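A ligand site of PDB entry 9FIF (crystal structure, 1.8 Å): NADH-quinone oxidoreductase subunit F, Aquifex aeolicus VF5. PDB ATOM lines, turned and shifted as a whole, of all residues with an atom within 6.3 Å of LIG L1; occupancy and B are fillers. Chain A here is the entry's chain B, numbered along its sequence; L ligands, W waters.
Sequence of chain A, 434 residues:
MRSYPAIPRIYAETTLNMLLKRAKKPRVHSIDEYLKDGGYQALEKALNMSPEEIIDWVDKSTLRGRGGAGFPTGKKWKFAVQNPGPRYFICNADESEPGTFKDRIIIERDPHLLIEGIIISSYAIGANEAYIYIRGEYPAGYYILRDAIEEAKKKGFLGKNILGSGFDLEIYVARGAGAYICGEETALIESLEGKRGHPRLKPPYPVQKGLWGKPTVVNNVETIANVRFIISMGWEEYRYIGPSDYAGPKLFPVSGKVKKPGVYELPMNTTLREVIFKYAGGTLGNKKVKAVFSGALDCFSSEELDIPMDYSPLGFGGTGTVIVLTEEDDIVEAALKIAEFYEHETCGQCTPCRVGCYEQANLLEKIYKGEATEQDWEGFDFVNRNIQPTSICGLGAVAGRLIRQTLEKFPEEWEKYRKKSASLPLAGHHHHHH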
ATOM      1  N   GLY A  67      23.873   6.018   4.616  1.00  0.00           N
ATOM      2  CA  GLY A  67      24.722   6.959   3.892  1.00  0.00           C
ATOM      3  C   GLY A  67      25.069   8.187   4.735  1.00  0.00           C
ATOM      4  O   GLY A  67      25.723   9.094   4.234  1.00  0.00           O
ATOM      5  N   GLY A  68      24.610   8.220   5.993  1.00  0.00           N
ATOM      6  CA  GLY A  68      25.127   9.220   6.919  1.00  0.00           C
ATOM      7  C   GLY A  68      24.047   9.974   7.671  1.00  0.00           C
ATOM      8  O   GLY A  68      24.294  10.452   8.774  1.00  0.00           O
ATOM      9  N   ALA A  69      22.865  10.134   7.078  1.00  0.00           N
ATOM     10  CA  ALA A  69      21.830  10.956   7.682  1.00  0.00           C
ATOM     11  C   ALA A  69      20.822  10.111   8.479  1.00  0.00           C
ATOM     12  O   ALA A  69      19.993  10.675   9.183  1.00  0.00           O
ATOM     13  CB  ALA A  69      21.142  11.755   6.616  1.00  0.00           C
ATOM     14  N   GLY A  70      20.838   8.782   8.297  1.00  0.00           N
ATOM     15  CA  GLY A  70      20.034   7.874   9.097  1.00  0.00           C
ATOM     16  C   GLY A  70      18.529   8.107   8.981  1.00  0.00           C
ATOM     17  O   GLY A  70      17.794   7.825   9.909  1.00  0.00           O
ATOM     18  N   PHE A  71      18.041   8.565   7.813  1.00  0.00           N
ATOM     19  CA  PHE A  71      16.616   8.717   7.615  1.00  0.00           C
ATOM     20  C   PHE A  71      15.934   7.347   7.485  1.00  0.00           C
ATOM     21  O   PHE A  71      16.448   6.446   6.819  1.00  0.00           O
ATOM     22  CB  PHE A  71      16.331   9.579   6.396  1.00  0.00           C
ATOM     23  CG  PHE A  71      14.907  10.087   6.416  1.00  0.00           C
ATOM     24  CD1 PHE A  71      13.880   9.344   5.838  1.00  0.00           C
ATOM     25  CD2 PHE A  71      14.582  11.285   7.048  1.00  0.00           C
ATOM     26  CE1 PHE A  71      12.576   9.794   5.876  1.00  0.00           C
ATOM     27  CE2 PHE A  71      13.270  11.736   7.080  1.00  0.00           C
ATOM     28  CZ  PHE A  71      12.271  10.991   6.497  1.00  0.00           C
ATOM     29  N   PRO A  72      14.776   7.106   8.146  1.00  0.00           N
ATOM     30  CA  PRO A  72      14.097   5.809   8.048  1.00  0.00           C
ATOM     31  C   PRO A  72      13.690   5.461   6.621  1.00  0.00           C
ATOM     32  O   PRO A  72      13.018   6.255   5.948  1.00  0.00           O
ATOM     33  CB  PRO A  72      12.889   5.952   8.999  1.00  0.00           C
ATOM     34  CG  PRO A  72      13.279   7.091   9.918  1.00  0.00           C
ATOM     35  CD  PRO A  72      14.082   8.035   9.051  1.00  0.00           C
ATOM     36  N   LYS A  75       9.887   5.019   5.527  1.00  0.00           N
ATOM     37  CA  LYS A  75       9.214   6.320   5.545  1.00  0.00           C
ATOM     38  C   LYS A  75       9.565   7.108   4.291  1.00  0.00           C
ATOM     39  O   LYS A  75       8.671   7.741   3.701  1.00  0.00           O
ATOM     40  CB  LYS A  75       9.521   7.116   6.814  1.00  0.00           C
ATOM     41  CG  LYS A  75       8.597   6.700   7.955  1.00  0.00           C
ATOM     42  CD  LYS A  75       8.822   7.377   9.302  1.00  0.00           C
ATOM     43  CE  LYS A  75       7.686   7.082  10.243  1.00  0.00           C
ATOM     44  NZ  LYS A  75       7.356   5.650  10.270  1.00  0.00           N
ATOM     45  N   LYS A  76      10.830   7.006   3.867  1.00  0.00           N
ATOM     46  CA  LYS A  76      11.277   7.669   2.646  1.00  0.00           C
ATOM     47  C   LYS A  76      10.490   7.140   1.439  1.00  0.00           C
ATOM     48  O   LYS A  76      10.020   7.920   0.602  1.00  0.00           O
ATOM     49  CB  LYS A  76      12.769   7.494   2.402  1.00  0.00           C
ATOM     50  CG  LYS A  76      13.302   8.380   1.290  1.00  0.00           C
ATOM     51  CD  LYS A  76      14.745   8.107   0.887  1.00  0.00           C
ATOM     52  CE  LYS A  76      15.706   8.207   2.008  1.00  0.00           C
ATOM     53  NZ  LYS A  76      17.085   8.243   1.513  1.00  0.00           N
ATOM     54  N   PHE A  79       6.912   8.267   1.371  1.00  0.00           N
ATOM     55  CA  PHE A  79       6.778   9.653   0.924  1.00  0.00           C
ATOM     56  C   PHE A  79       6.781   9.722  -0.604  1.00  0.00           C
ATOM     57  O   PHE A  79       5.959  10.431  -1.189  1.00  0.00           O
ATOM     58  CB  PHE A  79       7.867  10.552   1.504  1.00  0.00           C
ATOM     59  CG  PHE A  79       7.658  10.973   2.956  1.00  0.00           C
ATOM     60  CD1 PHE A  79       6.398  11.270   3.447  1.00  0.00           C
ATOM     61  CD2 PHE A  79       8.735  11.070   3.826  1.00  0.00           C
ATOM     62  CE1 PHE A  79       6.215  11.651   4.774  1.00  0.00           C
ATOM     63  CE2 PHE A  79       8.559  11.459   5.144  1.00  0.00           C
ATOM     64  CZ  PHE A  79       7.301  11.735   5.615  1.00  0.00           C
ATOM     65  N   GLY A 183      28.100  12.829  -4.069  1.00  0.00           N
ATOM     66  CA  GLY A 183      27.437  11.931  -3.121  1.00  0.00           C
ATOM     67  C   GLY A 183      26.212  12.549  -2.444  1.00  0.00           C
ATOM     68  O   GLY A 183      25.342  11.826  -1.944  1.00  0.00           O
ATOM     69  N   GLU A 184      26.171  13.883  -2.365  1.00  0.00           N
ATOM     70  CA  GLU A 184      24.989  14.575  -1.887  1.00  0.00           C
ATOM     71  C   GLU A 184      23.877  14.331  -2.902  1.00  0.00           C
ATOM     72  O   GLU A 184      24.067  14.511  -4.102  1.00  0.00           O
ATOM     73  CB  GLU A 184      25.303  16.061  -1.735  1.00  0.00           C
ATOM     74  CG  GLU A 184      24.286  16.799  -0.864  1.00  0.00           C
ATOM     75  CD  GLU A 184      22.992  17.275  -1.498  1.00  0.00           C
ATOM     76  OE1 GLU A 184      22.856  17.293  -2.726  1.00  0.00           O
ATOM     77  OE2 GLU A 184      22.084  17.648  -0.705  1.00  0.00           O
ATOM     78  N   GLU A 185      22.708  13.888  -2.422  1.00  0.00           N
ATOM     79  CA  GLU A 185      21.719  13.254  -3.293  1.00  0.00           C
ATOM     80  C   GLU A 185      21.239  14.208  -4.389  1.00  0.00           C
ATOM     81  O   GLU A 185      21.012  13.767  -5.519  1.00  0.00           O
ATOM     82  CB  GLU A 185      20.546  12.711  -2.497  1.00  0.00           C
ATOM     83  CG  GLU A 185      19.807  13.796  -1.715  1.00  0.00           C
ATOM     84  CD  GLU A 185      18.651  13.327  -0.855  1.00  0.00           C
ATOM     85  OE1 GLU A 185      18.315  12.141  -0.897  1.00  0.00           O
ATOM     86  OE2 GLU A 185      18.122  14.193  -0.134  1.00  0.00           O
ATOM     87  N   LYS A 202      16.885  22.542  -0.730  1.00  0.00           N
ATOM     88  CA  LYS A 202      15.854  21.660  -0.214  1.00  0.00           C
ATOM     89  C   LYS A 202      15.108  22.395   0.897  1.00  0.00           C
ATOM     90  O   LYS A 202      15.712  23.167   1.641  1.00  0.00           O
ATOM     91  CB  LYS A 202      16.456  20.382   0.354  1.00  0.00           C
ATOM     92  CG  LYS A 202      17.340  19.578  -0.591  1.00  0.00           C
ATOM     93  CD  LYS A 202      17.919  18.338   0.079  1.00  0.00           C
ATOM     94  CE  LYS A 202      18.603  18.649   1.373  1.00  0.00           C
ATOM     95  NZ  LYS A 202      18.677  17.477   2.258  1.00  0.00           N
ATOM     96  N   TYR A 205      12.408  17.922  -1.422  1.00  0.00           N
ATOM     97  CA  TYR A 205      13.257  16.749  -1.306  1.00  0.00           C
ATOM     98  C   TYR A 205      13.071  15.924  -2.572  1.00  0.00           C
ATOM     99  O   TYR A 205      12.023  15.991  -3.220  1.00  0.00           O
ATOM    100  CB  TYR A 205      12.944  15.949  -0.036  1.00  0.00           C
ATOM    101  CG  TYR A 205      13.343  16.661   1.258  1.00  0.00           C
ATOM    102  CD1 TYR A 205      12.462  17.515   1.905  1.00  0.00           C
ATOM    103  CD2 TYR A 205      14.610  16.473   1.816  1.00  0.00           C
ATOM    104  CE1 TYR A 205      12.821  18.171   3.079  1.00  0.00           C
ATOM    105  CE2 TYR A 205      14.983  17.118   2.988  1.00  0.00           C
ATOM    106  CZ  TYR A 205      14.091  17.972   3.615  1.00  0.00           C
ATOM    107  OH  TYR A 205      14.452  18.596   4.769  1.00  0.00           O
ATOM    108  N   PRO A 206      14.087  15.128  -2.959  1.00  0.00           N
ATOM    109  CA  PRO A 206      14.019  14.310  -4.167  1.00  0.00           C
ATOM    110  C   PRO A 206      12.747  13.473  -4.281  1.00  0.00           C
ATOM    111  O   PRO A 206      12.288  13.240  -5.388  1.00  0.00           O
ATOM    112  CB  PRO A 206      15.271  13.431  -4.058  1.00  0.00           C
ATOM    113  CG  PRO A 206      16.252  14.309  -3.307  1.00  0.00           C
ATOM    114  CD  PRO A 206      15.402  15.035  -2.292  1.00  0.00           C
ATOM    115  N   VAL A 207      12.194  13.022  -3.146  1.00  0.00           N
ATOM    116  CA  VAL A 207      11.036  12.134  -3.161  1.00  0.00           C
ATOM    117  C   VAL A 207       9.812  12.872  -3.713  1.00  0.00           C
ATOM    118  O   VAL A 207       8.855  12.217  -4.093  1.00  0.00           O
ATOM    119  CB  VAL A 207      10.726  11.522  -1.787  1.00  0.00           C
ATOM    120  CG1 VAL A 207      11.778  10.493  -1.398  1.00  0.00           C
ATOM    121  CG2 VAL A 207      10.546  12.598  -0.721  1.00  0.00           C
ATOM    122  N   VAL A 218      16.628   8.138  -3.440  1.00  0.00           N
ATOM    123  CA  VAL A 218      18.043   7.868  -3.371  1.00  0.00           C
ATOM    124  C   VAL A 218      18.318   7.101  -2.084  1.00  0.00           C
ATOM    125  O   VAL A 218      17.879   7.542  -1.017  1.00  0.00           O
ATOM    126  CB  VAL A 218      18.867   9.168  -3.392  1.00  0.00           C
ATOM    127  CG1 VAL A 218      20.365   8.886  -3.423  1.00  0.00           C
ATOM    128  CG2 VAL A 218      18.443  10.064  -4.552  1.00  0.00           C
ATOM    129  N   ASN A 219      18.984   5.944  -2.209  1.00  0.00           N
ATOM    130  CA  ASN A 219      19.457   5.164  -1.064  1.00  0.00           C
ATOM    131  C   ASN A 219      20.907   4.753  -1.273  1.00  0.00           C
ATOM    132  O   ASN A 219      21.358   4.479  -2.387  1.00  0.00           O
ATOM    133  CB  ASN A 219      18.599   3.935  -0.768  1.00  0.00           C
ATOM    134  CG  ASN A 219      17.384   4.232   0.075  1.00  0.00           C
ATOM    135  OD1 ASN A 219      17.488   4.742   1.208  1.00  0.00           O
ATOM    136  ND2 ASN A 219      16.219   3.913  -0.451  1.00  0.00           N
ATOM    137  N   CYS A 393      23.672  22.795   1.578  1.00  0.00           N
ATOM    138  CA  CYS A 393      23.858  21.359   1.760  1.00  0.00           C
ATOM    139  C   CYS A 393      24.698  21.094   3.007  1.00  0.00           C
ATOM    140  O   CYS A 393      25.234  22.003   3.626  1.00  0.00           O
ATOM    141  CB  CYS A 393      24.412  20.658   0.522  1.00  0.00           C
ATOM    142  SG  CYS A 393      26.221  20.529   0.385  1.00  0.00           S
ATOM    143  N   GLY A 394      24.816  19.804   3.359  1.00  0.00           N
ATOM    144  CA  GLY A 394      25.467  19.369   4.591  1.00  0.00           C
ATOM    145  C   GLY A 394      26.970  19.624   4.638  1.00  0.00           C
ATOM    146  O   GLY A 394      27.520  19.680   5.732  1.00  0.00           O
HETATM  147  P1  LIG L   1      19.532  14.611   5.197  1.00  0.00           P
HETATM  148  O1  LIG L   1      19.331  14.650   6.660  1.00  0.00           O
HETATM  149  O2  LIG L   1      19.074  15.859   4.476  1.00  0.00           O
HETATM  150  O3  LIG L   1      18.888  13.392   4.340  1.00  0.00           O
HETATM  151  C1  LIG L   1      18.378  12.133   4.836  1.00  0.00           C
HETATM  152  C2  LIG L   1      17.673  11.404   3.733  1.00  0.00           C
HETATM  153  O4  LIG L   1      16.252  11.437   4.030  1.00  0.00           O
HETATM  154  C3  LIG L   1      17.790  11.987   2.337  1.00  0.00           C
HETATM  155  O5  LIG L   1      17.515  10.996   1.346  1.00  0.00           O
HETATM  156  C4  LIG L   1      16.676  13.035   2.331  1.00  0.00           C
HETATM  157  O6  LIG L   1      16.137  13.297   1.038  1.00  0.00           O
HETATM  158  C5  LIG L   1      15.582  12.296   3.130  1.00  0.00           C
HETATM  159  N1  LIG L   1      14.694  13.169   3.892  1.00  0.00           N
HETATM  160  C6  LIG L   1      14.991  13.915   5.000  1.00  0.00           C
HETATM  161  N2  LIG L   1      13.969  14.578   5.495  1.00  0.00           N
HETATM  162  C7  LIG L   1      12.919  14.231   4.648  1.00  0.00           C
HETATM  163  C8  LIG L   1      11.563  14.581   4.636  1.00  0.00           C
HETATM  164  N3  LIG L   1      10.989  15.382   5.541  1.00  0.00           N
HETATM  165  N4  LIG L   1      10.788  14.066   3.657  1.00  0.00           N
HETATM  166  C9  LIG L   1      11.349  13.237   2.770  1.00  0.00           C
HETATM  167  N5  LIG L   1      12.612  12.826   2.686  1.00  0.00           N
HETATM  168  C10 LIG L   1      13.359  13.363   3.655  1.00  0.00           C
HETATM  169  O7  LIG L   1      21.092  14.408   4.906  1.00  0.00           O
HETATM  170  P2  LIG L   1      22.144  14.724   3.756  1.00  0.00           P
HETATM  171  O8  LIG L   1      22.444  16.228   3.860  1.00  0.00           O
HETATM  172  O9  LIG L   1      21.745  14.291   2.419  1.00  0.00           O
HETATM  173  O10 LIG L   1      23.426  13.834   4.342  1.00  0.00           O
HETATM  174  C11 LIG L   1      24.430  14.036   5.371  1.00  0.00           C
HETATM  175  C12 LIG L   1      25.329  12.814   5.417  1.00  0.00           C
HETATM  176  N1  LG2 L   2      25.308   9.200   0.699  1.00  0.00           N
HETATM  177  C1  LG2 L   2      25.753   8.038   0.124  1.00  0.00           C
HETATM  178  O1  LG2 L   2      25.023   7.054   0.003  1.00  0.00           O
HETATM  179  N2  LG2 L   2      27.028   8.061  -0.381  1.00  0.00           N
HETATM  180  C2  LG2 L   2      27.897   9.148  -0.383  1.00  0.00           C
HETATM  181  O2  LG2 L   2      29.007   9.020  -0.901  1.00  0.00           O
HETATM  182  C3  LG2 L   2      27.350  10.339   0.216  1.00  0.00           C
HETATM  183  N3  LG2 L   2      28.084  11.484   0.198  1.00  0.00           N
HETATM  184  C4  LG2 L   2      27.533  12.687   0.682  1.00  0.00           C
HETATM  185  C5  LG2 L   2      28.267  13.869   0.612  1.00  0.00           C
HETATM  186  C6  LG2 L   2      27.746  15.061   1.105  1.00  0.00           C
HETATM  187  C7  LG2 L   2      28.573  16.327   1.029  1.00  0.00           C
HETATM  188  C8  LG2 L   2      26.465  15.064   1.689  1.00  0.00           C
HETATM  189  C9  LG2 L   2      25.909  16.299   2.337  1.00  0.00           C
HETATM  190  C10 LG2 L   2      25.728  13.882   1.745  1.00  0.00           C
HETATM  191  C11 LG2 L   2      26.250  12.700   1.251  1.00  0.00           C
HETATM  192  N4  LG2 L   2      25.508  11.476   1.296  1.00  0.00           N
HETATM  193  C12 LG2 L   2      26.075  10.338   0.755  1.00  0.00           C
HETATM  194  C13 LG2 L   2      24.147  11.453   1.851  1.00  0.00           C
HETATM  195  C14 LG2 L   2      23.111  11.517   0.721  1.00  0.00           C
HETATM  196  O3  LG2 L   2      22.830  12.880   0.394  1.00  0.00           O
HETATM  197  C15 LG2 L   2      21.822  10.806   1.121  1.00  0.00           C
HETATM  198  O4  LG2 L   2      21.360  11.163   2.426  1.00  0.00           O
HETATM  199  C16 LG2 L   2      21.859   9.270   1.025  1.00  0.00           C
HETATM  200  O5  LG2 L   2      22.449   8.790  -0.188  1.00  0.00           O
HETATM  201  C17 LG2 L   2      20.464   8.721   1.198  1.00  0.00           C
HETATM  202  O6  LG2 L   2      20.467   7.268   1.241  1.00  0.00           O
HETATM  203  P1  LG2 L   2      20.238   6.564   2.670  1.00  0.00           P
HETATM  204  O7  LG2 L   2      18.934   7.098   3.214  1.00  0.00           O
HETATM  205  O8  LG2 L   2      20.172   5.095   2.273  1.00  0.00           O
HETATM  206  O9  LG2 L   2      21.433   6.893   3.536  1.00  0.00           O
HETATM  207  O   HOH W   1      14.197  12.433  -0.157  1.00  0.00           O
HETATM  208  O   HOH W   2      26.071  16.626   6.554  1.00  0.00           O
HETATM  209  O   HOH W   3      22.700  17.999   2.195  1.00  0.00           O
HETATM  210  O   HOH W   4      19.212   8.820   5.243  1.00  0.00           O
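The side-chain carboxylate (OE2) of Glu 185 is in hydrogen-bond range of an oxygen (O6) of LIG L1. O2 of LIG L1 lies within salt-bridge range of NZ of Lys 202 (2.8 Å). The side-chain amino group of Lys 76 is in hydrogen-bond range of an oxygen (O5) of LIG L1 (2.8 Å). An oxygen (O3) of LG2 L2 sits at hydrogen-bond distance from the backbone NH of Glu 185, at 3.0 Å. The side-chain amino group (NZ) of Lys 76 is in salt-bridge range of an oxygen (O7) of LG2 L2, at 2.8 Å. The backbone NH (N) of Gly 67 sits at hydrogen-bond distance from an oxygen (O9) of LG2 L2, 2.8 Å away. O8 of LG2 L2 lies close to OD1 of Asn 219 (2.9 Å).
O9 of LIG L1 is in hydrogen-bond range of O3 of LG2 L2 (2.7 Å).
The backbone carbonyl oxygen (O) of Val 218 lies within hydrogen-bond range of the side-chain amino group (NZ) of Lys 76 (2.7 Å).
Merely in contact with LIG L1: Gly 67, Gly 68, Ala 69, Phe 71, Phe 79, Tyr 205, Pro 206 and Val 207. Within 4 Å of LIG L1: Gly 67, Gly 68, Ala 69, Phe 71, Lys 76, Phe 79, Glu 185, Lys 202, Tyr 205, Pro 206 and Val 207.
Water W3 lies within hydrogen-bond range of an oxygen (O8) of LIG L1 (2.4 Å), the side-chain carboxylate (OE2) of Glu 184 (3.0 Å) and the backbone NH (N) of Gly 394 (3.0 Å). Water W4 lies within hydrogen-bond range of an oxygen (O7) of LG2 L2 (2.7 Å), the backbone NH of Phe 71 (2.8 Å) and the backbone NH of Gly 70 (3.5 Å).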
